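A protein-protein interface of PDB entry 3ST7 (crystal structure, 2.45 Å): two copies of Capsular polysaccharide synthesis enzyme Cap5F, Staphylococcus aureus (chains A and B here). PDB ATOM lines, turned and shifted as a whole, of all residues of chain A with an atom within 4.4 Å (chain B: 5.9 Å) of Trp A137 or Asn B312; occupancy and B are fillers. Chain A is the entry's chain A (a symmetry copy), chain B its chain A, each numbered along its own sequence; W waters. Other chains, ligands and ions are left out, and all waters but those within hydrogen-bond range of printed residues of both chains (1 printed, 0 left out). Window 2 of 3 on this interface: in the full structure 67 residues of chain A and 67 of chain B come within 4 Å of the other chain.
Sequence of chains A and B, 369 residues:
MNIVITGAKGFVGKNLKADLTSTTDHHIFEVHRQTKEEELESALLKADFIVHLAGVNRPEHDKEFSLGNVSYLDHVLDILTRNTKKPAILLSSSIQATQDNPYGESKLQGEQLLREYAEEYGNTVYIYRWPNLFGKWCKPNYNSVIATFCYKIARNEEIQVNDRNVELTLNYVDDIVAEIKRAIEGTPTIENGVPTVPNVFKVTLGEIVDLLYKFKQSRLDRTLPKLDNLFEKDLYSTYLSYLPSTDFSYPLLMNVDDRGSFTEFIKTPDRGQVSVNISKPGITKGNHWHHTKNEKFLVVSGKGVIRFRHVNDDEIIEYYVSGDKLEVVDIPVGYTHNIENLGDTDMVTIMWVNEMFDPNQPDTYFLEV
A ring nitrogen (ND1) of His B291 sits at hydrogen-bond distance from the side-chain amino group (NZ) of Lys A136. NE1 of Trp A137 is in hydrogen-bond range of NE2 of His B310 (3.3 Å).
NE2 of His B310 sits at hydrogen-bond distance from ND2 of Asn B312. O of Gly B334 is in hydrogen-bond range of N of Val B311, at 3.1 Å. O of Phe A11 is in hydrogen-bond range of ND2 of Asn A15 (3.0 Å). The side-chain amino group (NZ) of Lys A14 is in hydrogen-bond range of the backbone carbonyl oxygen (O) of Trp A137 (3.4 Å). The side-chain amide oxygen (OD1) of Asn A15 lies within hydrogen-bond range of the side-chain amino group (NZ) of Lys A136, at 2.8 Å.
Among the printed residues, pairs that only touch across the chains: Asn A15 with His B291 (3.99 Å), Ala A18 with Trp B289 (3.8 Å), Lys A136 with Val B333 (3.7 Å), Lys A136 with Gly B334 (3.95 Å), Trp A137 with Asn B312 (3.9 Å) and Trp A137 with Gly B334 (3.9 Å).
Of the printed residues of chain B, Asn A15 touches His B291. Of the printed residues of chain B, Ala A18 touches Trp B289. Of chain B, only His B310, Asn B312 and Gly B334 come within 4 Å of Trp A137. Of the printed residues of chain A, Trp B289 touches Ala A18. Of the printed residues of chain A, His B310 touches Trp A137 (3.3 Å). Val B311 touches none of the printed residues of chain A. Printed residues of chain A within 4 Å of Asn B312: Trp A137. Of the printed residues of chain A, Gly B334 touches Lys A136 (3.95 Å) and Trp A137 (3.9 Å). Tyr B335 touches none of the printed residues of chain A. The nearest residue of chain A that does not touch Asn B312 is Lys A14 (4.2 Å). The nearest printed residue of chain B that does not touch Asn A15 is Trp B289 (5.6 Å).
Of the 10 printed residues of chain B, 6 touch a printed residue of chain A. Hydrophobic or aromatic side chains of chain B that line the printed part of chain A: Trp B289, His B291, His B310 and Val B333. Along chain B the printed residues that touch a printed residue of chain A span positions 289 to 334. Among the printed residues, no Asp or Glu carboxylate lies within 4 Å of a Lys or Arg side-chain nitrogen of the other chain.
No position is printed for both chains.
Water W1 lies within hydrogen-bond range of the backbone carbonyl oxygen of His B291 (2.7 Å) and the side-chain amino group of Lys A136 (2.8 Å).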
ATOM      1  N   PHE A  11     -10.849  12.788 -10.384  1.00  0.00           N
ATOM      2  CA  PHE A  11     -10.876  13.273  -9.011  1.00  0.00           C
ATOM      3  C   PHE A  11     -11.901  14.379  -8.765  1.00  0.00           C
ATOM      4  O   PHE A  11     -12.815  14.197  -7.972  1.00  0.00           O
ATOM      5  CB  PHE A  11      -9.426  13.690  -8.676  1.00  0.00           C
ATOM      6  CG  PHE A  11      -9.268  14.568  -7.497  1.00  0.00           C
ATOM      7  CD1 PHE A  11      -9.768  14.206  -6.258  1.00  0.00           C
ATOM      8  CD2 PHE A  11      -8.532  15.737  -7.614  1.00  0.00           C
ATOM      9  CE1 PHE A  11      -9.559  15.029  -5.146  1.00  0.00           C
ATOM     10  CE2 PHE A  11      -8.312  16.559  -6.507  1.00  0.00           C
ATOM     11  CZ  PHE A  11      -8.834  16.210  -5.271  1.00  0.00           C
ATOM     12  N   LYS A  14     -15.737  13.269  -9.864  1.00  0.00           N
ATOM     13  CA  LYS A  14     -16.400  12.403  -8.880  1.00  0.00           C
ATOM     14  C   LYS A  14     -16.871  13.221  -7.682  1.00  0.00           C
ATOM     15  O   LYS A  14     -17.992  13.050  -7.221  1.00  0.00           O
ATOM     16  CB  LYS A  14     -15.481  11.273  -8.404  1.00  0.00           C
ATOM     17  CG  LYS A  14     -14.944  10.347  -9.490  1.00  0.00           C
ATOM     18  CD  LYS A  14     -14.534   9.025  -8.870  1.00  0.00           C
ATOM     19  CE  LYS A  14     -13.248   8.425  -9.461  1.00  0.00           C
ATOM     20  NZ  LYS A  14     -12.008   8.876  -8.711  1.00  0.00           N
ATOM     21  N   ASN A  15     -16.012  14.116  -7.207  1.00  0.00           N
ATOM     22  CA  ASN A  15     -16.339  15.008  -6.107  1.00  0.00           C
ATOM     23  C   ASN A  15     -17.471  15.967  -6.404  1.00  0.00           C
ATOM     24  O   ASN A  15     -18.378  16.122  -5.584  1.00  0.00           O
ATOM     25  CB  ASN A  15     -15.098  15.792  -5.679  1.00  0.00           C
ATOM     26  CG  ASN A  15     -14.302  15.055  -4.611  1.00  0.00           C
ATOM     27  OD1 ASN A  15     -14.730  14.990  -3.468  1.00  0.00           O
ATOM     28  ND2 ASN A  15     -13.157  14.478  -4.987  1.00  0.00           N
ATOM     29  N   ALA A  18     -20.852  13.950  -6.804  1.00  0.00           N
ATOM     30  CA  ALA A  18     -21.439  13.537  -5.532  1.00  0.00           C
ATOM     31  C   ALA A  18     -22.131  14.715  -4.861  1.00  0.00           C
ATOM     32  O   ALA A  18     -23.273  14.583  -4.421  1.00  0.00           O
ATOM     33  CB  ALA A  18     -20.384  12.904  -4.601  1.00  0.00           C
ATOM     34  N   GLY A 135      -7.259  16.150  -2.104  1.00  0.00           N
ATOM     35  CA  GLY A 135      -8.526  15.883  -1.452  1.00  0.00           C
ATOM     36  C   GLY A 135      -8.844  14.431  -1.651  1.00  0.00           C
ATOM     37  O   GLY A 135      -8.103  13.728  -2.344  1.00  0.00           O
ATOM     38  N   LYS A 136      -9.933  13.970  -1.040  1.00  0.00           N
ATOM     39  CA  LYS A 136     -10.355  12.571  -1.156  1.00  0.00           C
ATOM     40  C   LYS A 136     -10.597  12.160  -2.627  1.00  0.00           C
ATOM     41  O   LYS A 136     -10.951  12.991  -3.453  1.00  0.00           O
ATOM     42  CB  LYS A 136     -11.614  12.313  -0.304  1.00  0.00           C
ATOM     43  CG  LYS A 136     -12.844  13.077  -0.723  1.00  0.00           C
ATOM     44  CD  LYS A 136     -13.969  12.873   0.262  1.00  0.00           C
ATOM     45  CE  LYS A 136     -15.321  13.420  -0.257  1.00  0.00           C
ATOM     46  NZ  LYS A 136     -15.187  14.805  -0.761  1.00  0.00           N
ATOM     47  N   TRP A 137     -10.400  10.878  -2.930  1.00  0.00           N
ATOM     48  CA  TRP A 137     -10.740  10.278  -4.233  1.00  0.00           C
ATOM     49  C   TRP A 137      -9.674  10.468  -5.314  1.00  0.00           C
ATOM     50  O   TRP A 137      -9.779   9.885  -6.373  1.00  0.00           O
ATOM     51  CB  TRP A 137     -12.167  10.641  -4.717  1.00  0.00           C
ATOM     52  CG  TRP A 137     -13.219  10.340  -3.673  1.00  0.00           C
ATOM     53  CD1 TRP A 137     -13.041   9.620  -2.512  1.00  0.00           C
ATOM     54  CD2 TRP A 137     -14.600  10.731  -3.685  1.00  0.00           C
ATOM     55  NE1 TRP A 137     -14.214   9.555  -1.813  1.00  0.00           N
ATOM     56  CE2 TRP A 137     -15.188  10.224  -2.504  1.00  0.00           C
ATOM     57  CE3 TRP A 137     -15.402  11.459  -4.576  1.00  0.00           C
ATOM     58  CZ2 TRP A 137     -16.543  10.413  -2.197  1.00  0.00           C
ATOM     59  CZ3 TRP A 137     -16.754  11.649  -4.262  1.00  0.00           C
ATOM     60  CH2 TRP A 137     -17.304  11.130  -3.081  1.00  0.00           C
ATOM     61  N   CYS A 138      -8.648  11.264  -5.033  1.00  0.00           N
ATOM     62  CA  CYS A 138      -7.489  11.363  -5.905  1.00  0.00           C
ATOM     63  C   CYS A 138      -6.757  10.023  -5.915  1.00  0.00           C
ATOM     64  O   CYS A 138      -6.445   9.485  -4.862  1.00  0.00           O
ATOM     65  CB  CYS A 138      -6.575  12.473  -5.406  1.00  0.00           C
ATOM     66  SG  CYS A 138      -5.297  13.011  -6.555  1.00  0.00           S
ATOM     67  N   LYS A 139      -6.517   9.473  -7.105  1.00  0.00           N
ATOM     68  CA  LYS A 139      -5.850   8.176  -7.290  1.00  0.00           C
ATOM     69  C   LYS A 139      -4.399   8.170  -6.757  1.00  0.00           C
ATOM     70  O   LYS A 139      -3.592   9.041  -7.105  1.00  0.00           O
ATOM     71  CB  LYS A 139      -5.866   7.823  -8.788  1.00  0.00           C
ATOM     72  CG  LYS A 139      -6.231   6.376  -9.150  1.00  0.00           C
ATOM     73  CD  LYS A 139      -5.073   5.388  -8.912  1.00  0.00           C
ATOM     74  CE  LYS A 139      -5.130   4.144  -9.840  1.00  0.00           C
ATOM     75  NZ  LYS A 139      -4.748   4.461 -11.270  1.00  0.00           N
ATOM     76  N   TYR A 242      -7.837   7.886   2.838  1.00  0.00           N
ATOM     77  CA  TYR A 242      -6.958   6.816   2.317  1.00  0.00           C
ATOM     78  C   TYR A 242      -6.763   5.610   3.238  1.00  0.00           C
ATOM     79  O   TYR A 242      -6.036   4.675   2.899  1.00  0.00           O
ATOM     80  CB  TYR A 242      -5.616   7.387   1.835  1.00  0.00           C
ATOM     81  CG  TYR A 242      -5.806   8.305   0.647  1.00  0.00           C
ATOM     82  CD1 TYR A 242      -5.919   7.791  -0.642  1.00  0.00           C
ATOM     83  CD2 TYR A 242      -5.921   9.686   0.820  1.00  0.00           C
ATOM     84  CE1 TYR A 242      -6.128   8.632  -1.731  1.00  0.00           C
ATOM     85  CE2 TYR A 242      -6.126  10.539  -0.261  1.00  0.00           C
ATOM     86  CZ  TYR A 242      -6.236  10.011  -1.533  1.00  0.00           C
ATOM     87  OH  TYR A 242      -6.436  10.849  -2.617  1.00  0.00           O
ATOM     88  N   TRP B 289     -23.084  11.198   4.802  1.00  0.00           N
ATOM     89  CA  TRP B 289     -21.642  11.355   4.643  1.00  0.00           C
ATOM     90  C   TRP B 289     -21.238  12.813   4.660  1.00  0.00           C
ATOM     91  O   TRP B 289     -22.097  13.702   4.621  1.00  0.00           O
ATOM     92  CB  TRP B 289     -21.133  10.691   3.365  1.00  0.00           C
ATOM     93  CG  TRP B 289     -21.741  11.209   2.095  1.00  0.00           C
ATOM     94  CD1 TRP B 289     -22.957  10.869   1.576  1.00  0.00           C
ATOM     95  CD2 TRP B 289     -21.157  12.129   1.170  1.00  0.00           C
ATOM     96  NE1 TRP B 289     -23.165  11.515   0.386  1.00  0.00           N
ATOM     97  CE2 TRP B 289     -22.078  12.303   0.114  1.00  0.00           C
ATOM     98  CE3 TRP B 289     -19.944  12.825   1.130  1.00  0.00           C
ATOM     99  CZ2 TRP B 289     -21.836  13.153  -0.967  1.00  0.00           C
ATOM    100  CZ3 TRP B 289     -19.700  13.681   0.056  1.00  0.00           C
ATOM    101  CH2 TRP B 289     -20.645  13.836  -0.978  1.00  0.00           C
ATOM    102  N   HIS B 291     -18.058  15.753   3.174  1.00  0.00           N
ATOM    103  CA  HIS B 291     -16.861  16.036   2.404  1.00  0.00           C
ATOM    104  C   HIS B 291     -15.634  16.146   3.309  1.00  0.00           C
ATOM    105  O   HIS B 291     -14.595  15.592   2.971  1.00  0.00           O
ATOM    106  CB  HIS B 291     -16.965  17.354   1.632  1.00  0.00           C
ATOM    107  CG  HIS B 291     -17.735  17.264   0.358  1.00  0.00           C
ATOM    108  ND1 HIS B 291     -17.514  16.284  -0.581  1.00  0.00           N
ATOM    109  CD2 HIS B 291     -18.675  18.082  -0.169  1.00  0.00           C
ATOM    110  CE1 HIS B 291     -18.313  16.478  -1.613  1.00  0.00           C
ATOM    111  NE2 HIS B 291     -19.029  17.563  -1.387  1.00  0.00           N
ATOM    112  N   HIS B 310     -18.564   3.410   1.182  1.00  0.00           N
ATOM    113  CA  HIS B 310     -18.031   4.440   0.294  1.00  0.00           C
ATOM    114  C   HIS B 310     -19.128   4.907  -0.651  1.00  0.00           C
ATOM    115  O   HIS B 310     -19.910   4.101  -1.152  1.00  0.00           O
ATOM    116  CB  HIS B 310     -16.861   3.875  -0.500  1.00  0.00           C
ATOM    117  CG  HIS B 310     -16.019   4.906  -1.188  1.00  0.00           C
ATOM    118  ND1 HIS B 310     -14.712   5.154  -0.826  1.00  0.00           N
ATOM    119  CD2 HIS B 310     -16.280   5.722  -2.236  1.00  0.00           C
ATOM    120  CE1 HIS B 310     -14.203   6.077  -1.621  1.00  0.00           C
ATOM    121  NE2 HIS B 310     -15.139   6.450  -2.473  1.00  0.00           N
ATOM    122  N   VAL B 311     -19.196   6.214  -0.869  1.00  0.00           N
ATOM    123  CA  VAL B 311     -20.232   6.816  -1.709  1.00  0.00           C
ATOM    124  C   VAL B 311     -20.291   6.202  -3.102  1.00  0.00           C
ATOM    125  O   VAL B 311     -21.399   5.907  -3.614  1.00  0.00           O
ATOM    126  CB  VAL B 311     -20.054   8.348  -1.779  1.00  0.00           C
ATOM    127  CG1 VAL B 311     -20.824   8.944  -2.938  1.00  0.00           C
ATOM    128  CG2 VAL B 311     -20.495   8.964  -0.478  1.00  0.00           C
ATOM    129  N   ASN B 312     -19.131   5.982  -3.725  1.00  0.00           N
ATOM    130  CA  ASN B 312     -19.137   5.423  -5.107  1.00  0.00           C
ATOM    131  C   ASN B 312     -19.251   3.881  -5.167  1.00  0.00           C
ATOM    132  O   ASN B 312     -18.978   3.289  -6.201  1.00  0.00           O
ATOM    133  CB  ASN B 312     -17.898   5.884  -5.910  1.00  0.00           C
ATOM    134  CG  ASN B 312     -17.615   7.400  -5.788  1.00  0.00           C
ATOM    135  OD1 ASN B 312     -18.473   8.231  -6.104  1.00  0.00           O
ATOM    136  ND2 ASN B 312     -16.390   7.750  -5.369  1.00  0.00           N
ATOM    137  N   ASP B 313     -19.670   3.244  -4.074  1.00  0.00           N
ATOM    138  CA  ASP B 313     -19.436   1.807  -3.876  1.00  0.00           C
ATOM    139  C   ASP B 313     -20.631   1.026  -3.317  1.00  0.00           C
ATOM    140  O   ASP B 313     -21.642   1.625  -2.940  1.00  0.00           O
ATOM    141  CB  ASP B 313     -18.247   1.623  -2.940  1.00  0.00           C
ATOM    142  CG  ASP B 313     -17.258   0.614  -3.454  1.00  0.00           C
ATOM    143  OD1 ASP B 313     -17.648  -0.565  -3.654  1.00  0.00           O
ATOM    144  OD2 ASP B 313     -16.085   1.011  -3.654  1.00  0.00           O
ATOM    145  N   ASP B 314     -20.482  -0.304  -3.249  1.00  0.00           N
ATOM    146  CA  ASP B 314     -21.546  -1.241  -2.847  1.00  0.00           C
ATOM    147  C   ASP B 314     -21.284  -1.962  -1.514  1.00  0.00           C
ATOM    148  O   ASP B 314     -22.222  -2.366  -0.821  1.00  0.00           O
ATOM    149  CB  ASP B 314     -21.763  -2.293  -3.952  1.00  0.00           C
ATOM    150  CG  ASP B 314     -22.605  -1.762  -5.116  1.00  0.00           C
ATOM    151  OD1 ASP B 314     -22.889  -2.542  -6.070  1.00  0.00           O
ATOM    152  OD2 ASP B 314     -22.991  -0.563  -5.084  1.00  0.00           O
ATOM    153  N   VAL B 333     -14.040  10.742   5.701  1.00  0.00           N
ATOM    154  CA  VAL B 333     -14.844  11.511   4.745  1.00  0.00           C
ATOM    155  C   VAL B 333     -15.128  10.699   3.505  1.00  0.00           C
ATOM    156  O   VAL B 333     -14.318   9.894   3.112  1.00  0.00           O
ATOM    157  CB  VAL B 333     -14.157  12.842   4.376  1.00  0.00           C
ATOM    158  CG1 VAL B 333     -14.056  13.721   5.613  1.00  0.00           C
ATOM    159  CG2 VAL B 333     -12.766  12.625   3.756  1.00  0.00           C
ATOM    160  N   GLY B 334     -16.295  10.888   2.908  1.00  0.00           N
ATOM    161  CA  GLY B 334     -16.648  10.220   1.651  1.00  0.00           C
ATOM    162  C   GLY B 334     -17.261   8.865   1.913  1.00  0.00           C
ATOM    163  O   GLY B 334     -17.679   8.178   0.985  1.00  0.00           O
ATOM    164  N   TYR B 335     -17.336   8.467   3.173  1.00  0.00           N
ATOM    165  CA  TYR B 335     -18.075   7.256   3.523  1.00  0.00           C
ATOM    166  C   TYR B 335     -19.374   7.646   4.197  1.00  0.00           C
ATOM    167  O   TYR B 335     -19.378   8.406   5.174  1.00  0.00           O
ATOM    168  CB  TYR B 335     -17.274   6.347   4.471  1.00  0.00           C
ATOM    169  CG  TYR B 335     -16.097   5.642   3.840  1.00  0.00           C
ATOM    170  CD1 TYR B 335     -14.873   6.286   3.715  1.00  0.00           C
ATOM    171  CD2 TYR B 335     -16.204   4.311   3.394  1.00  0.00           C
ATOM    172  CE1 TYR B 335     -13.778   5.644   3.150  1.00  0.00           C
ATOM    173  CE2 TYR B 335     -15.113   3.646   2.813  1.00  0.00           C
ATOM    174  CZ  TYR B 335     -13.899   4.322   2.689  1.00  0.00           C
ATOM    175  OH  TYR B 335     -12.798   3.709   2.119  1.00  0.00           O
HETATM  176  O   HOH W   1     -13.488  16.539   0.676  1.00  0.00           O
